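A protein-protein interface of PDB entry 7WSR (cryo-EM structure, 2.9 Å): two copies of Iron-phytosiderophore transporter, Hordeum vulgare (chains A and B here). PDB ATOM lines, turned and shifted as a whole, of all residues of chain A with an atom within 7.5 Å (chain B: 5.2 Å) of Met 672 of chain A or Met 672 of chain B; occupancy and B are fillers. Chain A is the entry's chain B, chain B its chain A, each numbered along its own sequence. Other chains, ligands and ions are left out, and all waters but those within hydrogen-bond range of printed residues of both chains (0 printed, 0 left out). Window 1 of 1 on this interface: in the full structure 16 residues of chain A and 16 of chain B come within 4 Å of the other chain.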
ATOM      1  N   TRP A 237      19.165  18.423 -14.479  1.00  0.00           N
ATOM      2  CA  TRP A 237      19.050  17.220 -13.666  1.00  0.00           C
ATOM      3  C   TRP A 237      19.711  17.408 -12.306  1.00  0.00           C
ATOM      4  O   TRP A 237      19.140  17.040 -11.275  1.00  0.00           O
ATOM      5  CB  TRP A 237      19.663  16.031 -14.404  1.00  0.00           C
ATOM      6  CG  TRP A 237      19.734  14.771 -13.595  1.00  0.00           C
ATOM      7  CD1 TRP A 237      20.852  14.047 -13.306  1.00  0.00           C
ATOM      8  CD2 TRP A 237      18.640  14.087 -12.973  1.00  0.00           C
ATOM      9  NE1 TRP A 237      20.525  12.955 -12.545  1.00  0.00           N
ATOM     10  CE2 TRP A 237      19.174  12.955 -12.324  1.00  0.00           C
ATOM     11  CE3 TRP A 237      17.263  14.318 -12.899  1.00  0.00           C
ATOM     12  CZ2 TRP A 237      18.378  12.061 -11.613  1.00  0.00           C
ATOM     13  CZ3 TRP A 237      16.480  13.431 -12.194  1.00  0.00           C
ATOM     14  CH2 TRP A 237      17.037  12.315 -11.560  1.00  0.00           C
ATOM     15  N   PHE A 240      17.560  19.774 -10.386  1.00  0.00           N
ATOM     16  CA  PHE A 240      16.349  19.127  -9.886  1.00  0.00           C
ATOM     17  C   PHE A 240      16.637  18.252  -8.673  1.00  0.00           C
ATOM     18  O   PHE A 240      15.840  18.216  -7.728  1.00  0.00           O
ATOM     19  CB  PHE A 240      15.702  18.307 -11.002  1.00  0.00           C
ATOM     20  CG  PHE A 240      14.483  17.548 -10.568  1.00  0.00           C
ATOM     21  CD1 PHE A 240      13.277  18.199 -10.381  1.00  0.00           C
ATOM     22  CD2 PHE A 240      14.541  16.182 -10.350  1.00  0.00           C
ATOM     23  CE1 PHE A 240      12.156  17.504  -9.981  1.00  0.00           C
ATOM     24  CE2 PHE A 240      13.424  15.483  -9.952  1.00  0.00           C
ATOM     25  CZ  PHE A 240      12.228  16.144  -9.766  1.00  0.00           C
ATOM     26  N   GLN A 241      17.766  17.538  -8.679  1.00  0.00           N
ATOM     27  CA  GLN A 241      18.090  16.652  -7.566  1.00  0.00           C
ATOM     28  C   GLN A 241      18.295  17.419  -6.269  1.00  0.00           C
ATOM     29  O   GLN A 241      18.136  16.855  -5.183  1.00  0.00           O
ATOM     30  CB  GLN A 241      19.349  15.843  -7.872  1.00  0.00           C
ATOM     31  CG  GLN A 241      19.230  14.861  -9.012  1.00  0.00           C
ATOM     32  CD  GLN A 241      20.524  14.105  -9.243  1.00  0.00           C
ATOM     33  OE1 GLN A 241      20.812  13.128  -8.557  1.00  0.00           O
ATOM     34  NE2 GLN A 241      21.315  14.565 -10.201  1.00  0.00           N
ATOM     35  N   PHE A 243      16.658  19.668  -4.655  1.00  0.00           N
ATOM     36  CA  PHE A 243      15.529  19.895  -3.763  1.00  0.00           C
ATOM     37  C   PHE A 243      15.169  18.679  -2.925  1.00  0.00           C
ATOM     38  O   PHE A 243      14.395  18.820  -1.971  1.00  0.00           O
ATOM     39  CB  PHE A 243      14.307  20.333  -4.571  1.00  0.00           C
ATOM     40  CG  PHE A 243      14.487  21.646  -5.272  1.00  0.00           C
ATOM     41  CD1 PHE A 243      14.284  22.837  -4.599  1.00  0.00           C
ATOM     42  CD2 PHE A 243      14.856  21.689  -6.602  1.00  0.00           C
ATOM     43  CE1 PHE A 243      14.447  24.045  -5.244  1.00  0.00           C
ATOM     44  CE2 PHE A 243      15.021  22.895  -7.250  1.00  0.00           C
ATOM     45  CZ  PHE A 243      14.817  24.073  -6.570  1.00  0.00           C
ATOM     46  N   TYR A 244      15.696  17.500  -3.245  1.00  0.00           N
ATOM     47  CA  TYR A 244      15.306  16.276  -2.560  1.00  0.00           C
ATOM     48  C   TYR A 244      16.437  15.631  -1.776  1.00  0.00           C
ATOM     49  O   TYR A 244      16.222  14.580  -1.162  1.00  0.00           O
ATOM     50  CB  TYR A 244      14.730  15.276  -3.570  1.00  0.00           C
ATOM     51  CG  TYR A 244      13.601  15.862  -4.381  1.00  0.00           C
ATOM     52  CD1 TYR A 244      12.323  15.959  -3.854  1.00  0.00           C
ATOM     53  CD2 TYR A 244      13.819  16.340  -5.666  1.00  0.00           C
ATOM     54  CE1 TYR A 244      11.292  16.503  -4.585  1.00  0.00           C
ATOM     55  CE2 TYR A 244      12.792  16.888  -6.404  1.00  0.00           C
ATOM     56  CZ  TYR A 244      11.532  16.967  -5.859  1.00  0.00           C
ATOM     57  OH  TYR A 244      10.506  17.510  -6.593  1.00  0.00           O
ATOM     58  N   THR A 245      17.627  16.221  -1.773  1.00  0.00           N
ATOM     59  CA  THR A 245      18.726  15.754  -0.928  1.00  0.00           C
ATOM     60  C   THR A 245      18.776  16.530   0.382  1.00  0.00           C
ATOM     61  O   THR A 245      19.793  17.117   0.743  1.00  0.00           O
ATOM     62  CB  THR A 245      20.045  15.864  -1.683  1.00  0.00           C
ATOM     63  OG1 THR A 245      20.301  17.236  -2.003  1.00  0.00           O
ATOM     64  CG2 THR A 245      19.991  15.064  -2.969  1.00  0.00           C
ATOM     65  N   GLY A 246      17.668  16.525   1.114  1.00  0.00           N
ATOM     66  CA  GLY A 246      17.538  17.357   2.292  1.00  0.00           C
ATOM     67  C   GLY A 246      17.706  16.627   3.606  1.00  0.00           C
ATOM     68  O   GLY A 246      16.946  16.856   4.548  1.00  0.00           O
ATOM     69  N   GLY A 247      18.696  15.748   3.681  1.00  0.00           N
ATOM     70  CA  GLY A 247      18.950  15.035   4.918  1.00  0.00           C
ATOM     71  C   GLY A 247      20.107  14.078   4.753  1.00  0.00           C
ATOM     72  O   GLY A 247      20.741  14.007   3.697  1.00  0.00           O
ATOM     73  N   ASP A 248      20.375  13.340   5.825  1.00  0.00           N
ATOM     74  CA  ASP A 248      21.434  12.341   5.808  1.00  0.00           C
ATOM     75  C   ASP A 248      20.989  11.125   5.005  1.00  0.00           C
ATOM     76  O   ASP A 248      20.054  10.418   5.398  1.00  0.00           O
ATOM     77  CB  ASP A 248      21.806  11.944   7.235  1.00  0.00           C
ATOM     78  CG  ASP A 248      20.589  11.735   8.118  1.00  0.00           C
ATOM     79  OD1 ASP A 248      19.465  12.039   7.667  1.00  0.00           O
ATOM     80  OD2 ASP A 248      20.757  11.268   9.263  1.00  0.00           O
ATOM     81  N   ALA A 249      21.655  10.891   3.874  1.00  0.00           N
ATOM     82  CA  ALA A 249      21.408   9.733   3.014  1.00  0.00           C
ATOM     83  C   ALA A 249      19.957   9.690   2.525  1.00  0.00           C
ATOM     84  O   ALA A 249      19.203   8.758   2.807  1.00  0.00           O
ATOM     85  CB  ALA A 249      21.788   8.432   3.728  1.00  0.00           C
ATOM     86  N   CYS A 250      19.580  10.725   1.776  1.00  0.00           N
ATOM     87  CA  CYS A 250      18.318  10.712   1.052  1.00  0.00           C
ATOM     88  C   CYS A 250      18.457  11.568  -0.198  1.00  0.00           C
ATOM     89  O   CYS A 250      19.132  12.598  -0.179  1.00  0.00           O
ATOM     90  CB  CYS A 250      17.142  11.200   1.907  1.00  0.00           C
ATOM     91  SG  CYS A 250      17.322  12.788   2.735  1.00  0.00           S
ATOM     92  N   GLY A 251      17.821  11.125  -1.274  1.00  0.00           N
ATOM     93  CA  GLY A 251      17.908  11.784  -2.562  1.00  0.00           C
ATOM     94  C   GLY A 251      18.217  10.794  -3.662  1.00  0.00           C
ATOM     95  O   GLY A 251      18.344   9.596  -3.399  1.00  0.00           O
ATOM     96  N   PHE A 252      18.341  11.273  -4.901  1.00  0.00           N
ATOM     97  CA  PHE A 252      18.702  10.381  -5.996  1.00  0.00           C
ATOM     98  C   PHE A 252      20.126   9.859  -5.867  1.00  0.00           C
ATOM     99  O   PHE A 252      20.449   8.826  -6.460  1.00  0.00           O
ATOM    100  CB  PHE A 252      18.531  11.088  -7.340  1.00  0.00           C
ATOM    101  CG  PHE A 252      17.111  11.127  -7.827  1.00  0.00           C
ATOM    102  CD1 PHE A 252      16.527  10.002  -8.380  1.00  0.00           C
ATOM    103  CD2 PHE A 252      16.365  12.287  -7.734  1.00  0.00           C
ATOM    104  CE1 PHE A 252      15.226  10.032  -8.829  1.00  0.00           C
ATOM    105  CE2 PHE A 252      15.062  12.323  -8.183  1.00  0.00           C
ATOM    106  CZ  PHE A 252      14.492  11.192  -8.730  1.00  0.00           C
ATOM    107  N   VAL A 253      20.983  10.550  -5.114  1.00  0.00           N
ATOM    108  CA  VAL A 253      22.345  10.072  -4.914  1.00  0.00           C
ATOM    109  C   VAL A 253      22.348   8.772  -4.115  1.00  0.00           C
ATOM    110  O   VAL A 253      23.092   7.839  -4.428  1.00  0.00           O
ATOM    111  CB  VAL A 253      23.204  11.166  -4.255  1.00  0.00           C
ATOM    112  CG1 VAL A 253      22.552  11.685  -2.978  1.00  0.00           C
ATOM    113  CG2 VAL A 253      24.606  10.651  -3.980  1.00  0.00           C
ATOM    114  N   GLN A 254      21.523   8.686  -3.077  1.00  0.00           N
ATOM    115  CA  GLN A 254      21.450   7.485  -2.246  1.00  0.00           C
ATOM    116  C   GLN A 254      20.261   6.617  -2.655  1.00  0.00           C
ATOM    117  O   GLN A 254      19.399   6.271  -1.848  1.00  0.00           O
ATOM    118  CB  GLN A 254      21.374   7.873  -0.772  1.00  0.00           C
ATOM    119  CG  GLN A 254      22.485   8.802  -0.323  1.00  0.00           C
ATOM    120  CD  GLN A 254      23.842   8.127  -0.298  1.00  0.00           C
ATOM    121  OE1 GLN A 254      23.939   6.904  -0.208  1.00  0.00           O
ATOM    122  NE2 GLN A 254      24.897   8.925  -0.381  1.00  0.00           N
ATOM    123  N   PHE A 255      20.231   6.251  -3.937  1.00  0.00           N
ATOM    124  CA  PHE A 255      19.117   5.503  -4.498  1.00  0.00           C
ATOM    125  C   PHE A 255      19.438   4.019  -4.495  1.00  0.00           C
ATOM    126  O   PHE A 255      20.405   3.606  -5.153  1.00  0.00           O
ATOM    127  CB  PHE A 255      18.814   5.974  -5.916  1.00  0.00           C
ATOM    128  CG  PHE A 255      17.405   5.697  -6.359  1.00  0.00           C
ATOM    129  CD1 PHE A 255      16.993   4.406  -6.649  1.00  0.00           C
ATOM    130  CD2 PHE A 255      16.495   6.728  -6.489  1.00  0.00           C
ATOM    131  CE1 PHE A 255      15.700   4.151  -7.053  1.00  0.00           C
ATOM    132  CE2 PHE A 255      15.198   6.475  -6.893  1.00  0.00           C
ATOM    133  CZ  PHE A 255      14.804   5.188  -7.176  1.00  0.00           C
ATOM    134  N   PRO A 256      18.673   3.185  -3.788  1.00  0.00           N
ATOM    135  CA  PRO A 256      18.901   1.724  -3.795  1.00  0.00           C
ATOM    136  C   PRO A 256      18.373   1.050  -5.057  1.00  0.00           C
ATOM    137  O   PRO A 256      17.316   0.424  -5.089  1.00  0.00           O
ATOM    138  CB  PRO A 256      18.141   1.259  -2.548  1.00  0.00           C
ATOM    139  CG  PRO A 256      17.743   2.505  -1.808  1.00  0.00           C
ATOM    140  CD  PRO A 256      17.629   3.569  -2.830  1.00  0.00           C
ATOM    141  N   ILE A 670      13.191  19.023   0.745  1.00  0.00           N
ATOM    142  CA  ILE A 670      12.612  17.693   0.855  1.00  0.00           C
ATOM    143  C   ILE A 670      13.735  16.673   0.995  1.00  0.00           C
ATOM    144  O   ILE A 670      14.873  16.908   0.593  1.00  0.00           O
ATOM    145  CB  ILE A 670      11.709  17.362  -0.356  1.00  0.00           C
ATOM    146  CG1 ILE A 670      10.834  18.568  -0.698  1.00  0.00           C
ATOM    147  CG2 ILE A 670      10.822  16.163  -0.076  1.00  0.00           C
ATOM    148  CD1 ILE A 670       9.936  18.358  -1.885  1.00  0.00           C
ATOM    149  N   CYS A 671      13.395  15.523   1.576  1.00  0.00           N
ATOM    150  CA  CYS A 671      14.329  14.427   1.808  1.00  0.00           C
ATOM    151  C   CYS A 671      13.685  13.136   1.326  1.00  0.00           C
ATOM    152  O   CYS A 671      12.722  12.658   1.932  1.00  0.00           O
ATOM    153  CB  CYS A 671      14.701  14.345   3.295  1.00  0.00           C
ATOM    154  SG  CYS A 671      15.645  12.899   3.878  1.00  0.00           S
ATOM    155  N   MET A 672      14.210  12.582   0.237  1.00  0.00           N
ATOM    156  CA  MET A 672      13.648  11.390  -0.399  1.00  0.00           C
ATOM    157  C   MET A 672      14.249  10.156   0.263  1.00  0.00           C
ATOM    158  O   MET A 672      15.292   9.656  -0.159  1.00  0.00           O
ATOM    159  CB  MET A 672      13.925  11.404  -1.896  1.00  0.00           C
ATOM    160  CG  MET A 672      13.380  10.205  -2.643  1.00  0.00           C
ATOM    161  SD  MET A 672      14.194   9.959  -4.232  1.00  0.00           S
ATOM    162  CE  MET A 672      14.168  11.626  -4.866  1.00  0.00           C
ATOM    163  N   LYS A 673      13.586   9.657   1.297  1.00  0.00           N
ATOM    164  CA  LYS A 673      14.075   8.527   2.072  1.00  0.00           C
ATOM    165  C   LYS A 673      13.502   7.219   1.538  1.00  0.00           C
ATOM    166  O   LYS A 673      12.377   7.160   1.040  1.00  0.00           O
ATOM    167  CB  LYS A 673      13.718   8.699   3.552  1.00  0.00           C
ATOM    168  CG  LYS A 673      14.443   7.747   4.480  1.00  0.00           C
ATOM    169  CD  LYS A 673      14.051   7.979   5.927  1.00  0.00           C
ATOM    170  CE  LYS A 673      14.419   9.379   6.382  1.00  0.00           C
ATOM    171  NZ  LYS A 673      14.038   9.615   7.801  1.00  0.00           N
ATOM    172  N   PHE A 674      14.304   6.161   1.645  1.00  0.00           N
ATOM    173  CA  PHE A 674      13.919   4.821   1.221  1.00  0.00           C
ATOM    174  C   PHE A 674      13.833   3.928   2.447  1.00  0.00           C
ATOM    175  O   PHE A 674      14.779   3.865   3.240  1.00  0.00           O
ATOM    176  CB  PHE A 674      14.916   4.256   0.210  1.00  0.00           C
ATOM    177  CG  PHE A 674      14.995   5.038  -1.066  1.00  0.00           C
ATOM    178  CD1 PHE A 674      15.783   6.172  -1.154  1.00  0.00           C
ATOM    179  CD2 PHE A 674      14.285   4.638  -2.179  1.00  0.00           C
ATOM    180  CE1 PHE A 674      15.857   6.891  -2.325  1.00  0.00           C
ATOM    181  CE2 PHE A 674      14.357   5.351  -3.352  1.00  0.00           C
ATOM    182  CZ  PHE A 674      15.143   6.479  -3.424  1.00  0.00           C
ATOM    183  N   LEU A 675      12.709   3.236   2.598  1.00  0.00           N
ATOM    184  CA  LEU A 675      12.461   2.392   3.751  1.00  0.00           C
ATOM    185  C   LEU A 675      12.054   0.992   3.308  1.00  0.00           C
ATOM    186  O   LEU A 675      11.473   0.821   2.234  1.00  0.00           O
ATOM    187  CB  LEU A 675      11.364   2.984   4.645  1.00  0.00           C
ATOM    188  CG  LEU A 675      11.654   4.315   5.342  1.00  0.00           C
ATOM    189  CD1 LEU A 675      11.302   5.494   4.451  1.00  0.00           C
ATOM    190  CD2 LEU A 675      10.906   4.397   6.663  1.00  0.00           C
ATOM    191  N   ALA A 677       9.655  -1.034   3.428  1.00  0.00           N
ATOM    192  CA  ALA A 677       8.217  -1.296   3.524  1.00  0.00           C
ATOM    193  C   ALA A 677       7.771  -1.439   4.974  1.00  0.00           C
ATOM    194  O   ALA A 677       6.986  -2.325   5.323  1.00  0.00           O
ATOM    195  CB  ALA A 677       7.825  -2.529   2.709  1.00  0.00           C
ATOM    196  N   TYR B 244       9.424   0.039  -5.679  1.00  0.00           N
ATOM    197  CA  TYR B 244       9.513   1.144  -4.736  1.00  0.00           C
ATOM    198  C   TYR B 244       8.160   1.702  -4.324  1.00  0.00           C
ATOM    199  O   TYR B 244       8.114   2.651  -3.533  1.00  0.00           O
ATOM    200  CB  TYR B 244      10.384   2.261  -5.323  1.00  0.00           C
ATOM    201  CG  TYR B 244      11.744   1.765  -5.751  1.00  0.00           C
ATOM    202  CD1 TYR B 244      12.752   1.562  -4.823  1.00  0.00           C
ATOM    203  CD2 TYR B 244      12.011   1.477  -7.083  1.00  0.00           C
ATOM    204  CE1 TYR B 244      13.989   1.097  -5.206  1.00  0.00           C
ATOM    205  CE2 TYR B 244      13.247   1.011  -7.475  1.00  0.00           C
ATOM    206  CZ  TYR B 244      14.231   0.825  -6.533  1.00  0.00           C
ATOM    207  OH  TYR B 244      15.466   0.363  -6.921  1.00  0.00           O
ATOM    208  N   ALA B 249       1.149   5.738  -0.303  1.00  0.00           N
ATOM    209  CA  ALA B 249       1.656   6.999  -0.848  1.00  0.00           C
ATOM    210  C   ALA B 249       3.184   7.072  -0.775  1.00  0.00           C
ATOM    211  O   ALA B 249       3.764   7.936  -0.115  1.00  0.00           O
ATOM    212  CB  ALA B 249       1.013   8.196  -0.142  1.00  0.00           C
ATOM    213  N   CYS B 250       3.831   6.143  -1.477  1.00  0.00           N
ATOM    214  CA  CYS B 250       5.267   6.224  -1.695  1.00  0.00           C
ATOM    215  C   CYS B 250       5.605   5.556  -3.018  1.00  0.00           C
ATOM    216  O   CYS B 250       4.995   4.551  -3.386  1.00  0.00           O
ATOM    217  CB  CYS B 250       6.072   5.591  -0.553  1.00  0.00           C
ATOM    218  SG  CYS B 250       5.650   3.908  -0.075  1.00  0.00           S
ATOM    219  N   GLY B 251       6.572   6.128  -3.723  1.00  0.00           N
ATOM    220  CA  GLY B 251       6.967   5.658  -5.036  1.00  0.00           C
ATOM    221  C   GLY B 251       7.045   6.801  -6.024  1.00  0.00           C
ATOM    222  O   GLY B 251       6.801   7.953  -5.659  1.00  0.00           O
ATOM    223  N   PHE B 252       7.384   6.503  -7.279  1.00  0.00           N
ATOM    224  CA  PHE B 252       7.414   7.548  -8.295  1.00  0.00           C
ATOM    225  C   PHE B 252       6.024   8.084  -8.611  1.00  0.00           C
ATOM    226  O   PHE B 252       5.907   9.198  -9.129  1.00  0.00           O
ATOM    227  CB  PHE B 252       8.071   7.033  -9.575  1.00  0.00           C
ATOM    228  CG  PHE B 252       9.572   7.025  -9.524  1.00  0.00           C
ATOM    229  CD1 PHE B 252      10.286   8.201  -9.668  1.00  0.00           C
ATOM    230  CD2 PHE B 252      10.265   5.844  -9.334  1.00  0.00           C
ATOM    231  CE1 PHE B 252      11.661   8.200  -9.624  1.00  0.00           C
ATOM    232  CE2 PHE B 252      11.644   5.838  -9.289  1.00  0.00           C
ATOM    233  CZ  PHE B 252      12.342   7.019  -9.432  1.00  0.00           C
ATOM    234  N   PHE B 255       5.144  11.388  -6.360  1.00  0.00           N
ATOM    235  CA  PHE B 255       6.365  12.178  -6.376  1.00  0.00           C
ATOM    236  C   PHE B 255       6.026  13.655  -6.281  1.00  0.00           C
ATOM    237  O   PHE B 255       5.347  14.181  -7.176  1.00  0.00           O
ATOM    238  CB  PHE B 255       7.166  11.903  -7.645  1.00  0.00           C
ATOM    239  CG  PHE B 255       8.632  12.202  -7.512  1.00  0.00           C
ATOM    240  CD1 PHE B 255       9.088  13.510  -7.453  1.00  0.00           C
ATOM    241  CD2 PHE B 255       9.556  11.176  -7.452  1.00  0.00           C
ATOM    242  CE1 PHE B 255      10.432  13.785  -7.328  1.00  0.00           C
ATOM    243  CE2 PHE B 255      10.904  11.449  -7.327  1.00  0.00           C
ATOM    244  CZ  PHE B 255      11.340  12.753  -7.268  1.00  0.00           C
ATOM    245  N   ILE B 670      10.380  -2.092  -1.313  1.00  0.00           N
ATOM    246  CA  ILE B 670      10.847  -0.806  -0.819  1.00  0.00           C
ATOM    247  C   ILE B 670       9.722   0.214  -0.947  1.00  0.00           C
ATOM    248  O   ILE B 670       8.809   0.066  -1.757  1.00  0.00           O
ATOM    249  CB  ILE B 670      12.114  -0.333  -1.569  1.00  0.00           C
ATOM    250  CG1 ILE B 670      13.084  -1.501  -1.741  1.00  0.00           C
ATOM    251  CG2 ILE B 670      12.811   0.792  -0.826  1.00  0.00           C
ATOM    252  CD1 ILE B 670      14.341  -1.151  -2.488  1.00  0.00           C
ATOM    253  N   CYS B 671       9.802   1.262  -0.128  1.00  0.00           N
ATOM    254  CA  CYS B 671       8.818   2.338  -0.093  1.00  0.00           C
ATOM    255  C   CYS B 671       9.559   3.666  -0.129  1.00  0.00           C
ATOM    256  O   CYS B 671      10.230   4.029   0.842  1.00  0.00           O
ATOM    257  CB  CYS B 671       7.939   2.220   1.158  1.00  0.00           C
ATOM    258  SG  CYS B 671       6.811   3.595   1.563  1.00  0.00           S
ATOM    259  N   MET B 672       9.442   4.381  -1.244  1.00  0.00           N
ATOM    260  CA  MET B 672      10.163   5.635  -1.464  1.00  0.00           C
ATOM    261  C   MET B 672       9.334   6.779  -0.894  1.00  0.00           C
ATOM    262  O   MET B 672       8.498   7.360  -1.586  1.00  0.00           O
ATOM    263  CB  MET B 672      10.439   5.838  -2.948  1.00  0.00           C
ATOM    264  CG  MET B 672      11.183   7.116  -3.276  1.00  0.00           C
ATOM    265  SD  MET B 672      10.983   7.602  -4.998  1.00  0.00           S
ATOM    266  CE  MET B 672      11.277   6.040  -5.808  1.00  0.00           C
ATOM    267  N   LYS B 673       9.571   7.111   0.367  1.00  0.00           N
ATOM    268  CA  LYS B 673       8.809   8.134   1.067  1.00  0.00           C
ATOM    269  C   LYS B 673       9.500   9.489   0.961  1.00  0.00           C
ATOM    270  O   LYS B 673      10.727   9.587   0.910  1.00  0.00           O
ATOM    271  CB  LYS B 673       8.619   7.747   2.537  1.00  0.00           C
ATOM    272  CG  LYS B 673       7.586   8.578   3.269  1.00  0.00           C
ATOM    273  CD  LYS B 673       7.442   8.137   4.713  1.00  0.00           C
ATOM    274  CE  LYS B 673       6.972   6.697   4.806  1.00  0.00           C
ATOM    275  NZ  LYS B 673       6.828   6.254   6.220  1.00  0.00           N
ATOM    276  N   PHE B 674       8.686  10.542   0.922  1.00  0.00           N
ATOM    277  CA  PHE B 674       9.162  11.917   0.855  1.00  0.00           C
ATOM    278  C   PHE B 674       8.781  12.628   2.143  1.00  0.00           C
ATOM    279  O   PHE B 674       7.614  12.603   2.547  1.00  0.00           O
ATOM    280  CB  PHE B 674       8.576  12.644  -0.355  1.00  0.00           C
ATOM    281  CG  PHE B 674       8.979  12.051  -1.671  1.00  0.00           C
ATOM    282  CD1 PHE B 674       8.304  10.961  -2.192  1.00  0.00           C
ATOM    283  CD2 PHE B 674      10.028  12.584  -2.390  1.00  0.00           C
ATOM    284  CE1 PHE B 674       8.670  10.416  -3.401  1.00  0.00           C
ATOM    285  CE2 PHE B 674      10.398  12.044  -3.599  1.00  0.00           C
ATOM    286  CZ  PHE B 674       9.718  10.958  -4.104  1.00  0.00           C
ATOM    287  N   LEU B 675       9.759  13.262   2.781  1.00  0.00           N
ATOM    288  CA  LEU B 675       9.558  13.930   4.052  1.00  0.00           C
ATOM    289  C   LEU B 675      10.060  15.367   3.985  1.00  0.00           C
ATOM    290  O   LEU B 675      10.981  15.672   3.224  1.00  0.00           O
ATOM    291  CB  LEU B 675      10.279  13.190   5.187  1.00  0.00           C
ATOM    292  CG  LEU B 675       9.794  11.783   5.541  1.00  0.00           C
ATOM    293  CD1 LEU B 675      10.471  10.732   4.678  1.00  0.00           C
ATOM    294  CD2 LEU B 675      10.024  11.497   7.017  1.00  0.00           C
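The side-chain hydroxyl (OH) of Tyr 244 of chain B is in hydrogen-bond range of the backbone carbonyl oxygen (O) of Pro 256 of chain A.
O of Leu 675 of chain A lies within hydrogen-bond range of N of Cys 671 of chain B (2.9 Å).
The backbone carbonyl oxygen of Lys 673 of chain B lies within hydrogen-bond range of the backbone NH of Lys 673 of chain A (2.9 Å).
The backbone NH of Cys 671 of chain A lies within hydrogen-bond range of the backbone carbonyl oxygen of Leu 675 of chain B, at 2.9 Å.
The backbone carbonyl oxygen (O) of Tyr 244 of chain B sits at hydrogen-bond distance from the backbone NH (N) of Met 672 of chain B.
The side-chain sulfur (SG) of Cys 250 of chain B forms a disulfide with the side-chain sulfur (SG) of Cys 671 of chain B (2.0 Å).
The backbone NH (N) of Gly 251 of chain B sits at hydrogen-bond distance from the backbone carbonyl oxygen (O) of Met 672 of chain B, 3.1 Å away.
The backbone NH (N) of Gly 246 of chain A lies within hydrogen-bond range of the backbone carbonyl oxygen (O) of Ile 670 of chain A, at 2.9 Å.
The side-chain sulfur of Cys 250 of chain A is disulfide-bonded to the side-chain sulfur of Cys 671 of chain A, 2.0 Å away.
The backbone carbonyl oxygen (O) of Met 672 of chain A sits at hydrogen-bond distance from the backbone NH (N) of Gly 251 of chain A, 3.1 Å away.
Tyr 244 of chain A touches Phe 255 of chain B.
Phe 252 of chain A touches Phe 255 of chain B.
Phe 252 of chain B touches Phe 255 of chain A.
CZ of Phe 255 of chain A touches CE of Met 672 of chain B, at 3.9 Å.
Ile 670 of chain A touches Leu 675 of chain B.
CE of Met 672 of chain A touches CZ of Phe 255 of chain B, at 3.9 Å.
O of Lys 673 of chain B touches C of Met 672 of chain A (3.6 Å).
Met 672 of chain B touches Lys 673 of chain A (C to O, 3.6 Å).
Met 672 of chain B touches Phe 674 of chain A (CG to CE2, 3.6 Å).
CG2 of Ile 670 of chain B touches O of Leu 675 of chain A, 3.3 Å away.
Of the printed residues of chain B, Met 672 of chain A touches Phe 255, Met 672, Lys 673 and Phe 674.
Printed residues of chain B within 4 Å of Lys 673 of chain A: Cys 671 (3.8 Å), Met 672 (3.6 Å), Lys 673 (2.9 Å) and Leu 675 (3.99 Å).
Ala 249 of chain B touches none of the printed residues of chain A.
Gly 251 of chain B touches none of the printed residues of chain A.
Of the printed residues of chain A, Phe 255 of chain B touches Phe 240 (3.8 Å), Tyr 244 (3.7 Å), Phe 252 (3.8 Å) and Met 672 (3.9 Å).
Met 672 of chain B touches just these residues of chain A: Phe 255 (3.9 Å), Met 672 (3.8 Å), Lys 673 (3.6 Å) and Phe 674 (3.6 Å).
Of the printed residues of chain A, Lys 673 of chain B touches Cys 671, Met 672, Lys 673 and Leu 675.
The nearest printed residue of chain B that does not touch Phe 240 of chain A is Phe 252 of chain B (7.5 Å).
Hydrophobic or aromatic side chains of chain A that line the printed part of chain B: Phe 240, Tyr 244, Phe 252, Phe 255, Ile 670, Met 672, Phe 674 and Leu 675.
Of the 12 printed residues of chain B, 9 touch a printed residue of chain A.
Hydrophobic or aromatic side chains of chain B that line the printed part of chain A: Tyr 244, Phe 252, Phe 255, Ile 670, Met 672, Phe 674 and Leu 675.
Among the printed residues, 24 pairs touch across the chains.
Tyr 244 of chain A touches Phe 255 of chain B, and with the chains exchanged Phe 255 of chain A touches Tyr 244 of chain B.
Phe 252 of chain A touches Phe 255 of chain B, and with the chains exchanged Phe 255 of chain A touches Phe 252 of chain B.
Cys 671 of chain A touches Phe 674 of chain B, and with the chains exchanged Phe 674 of chain A touches Cys 671 of chain B.
Met 672 of chain A touches Phe 674 of chain B, and with the chains exchanged Phe 674 of chain A touches Met 672 of chain B.
Of the 24 pairs that touch across the chains among the printed residues, 22 have their exchanged pair printed and touching as well.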
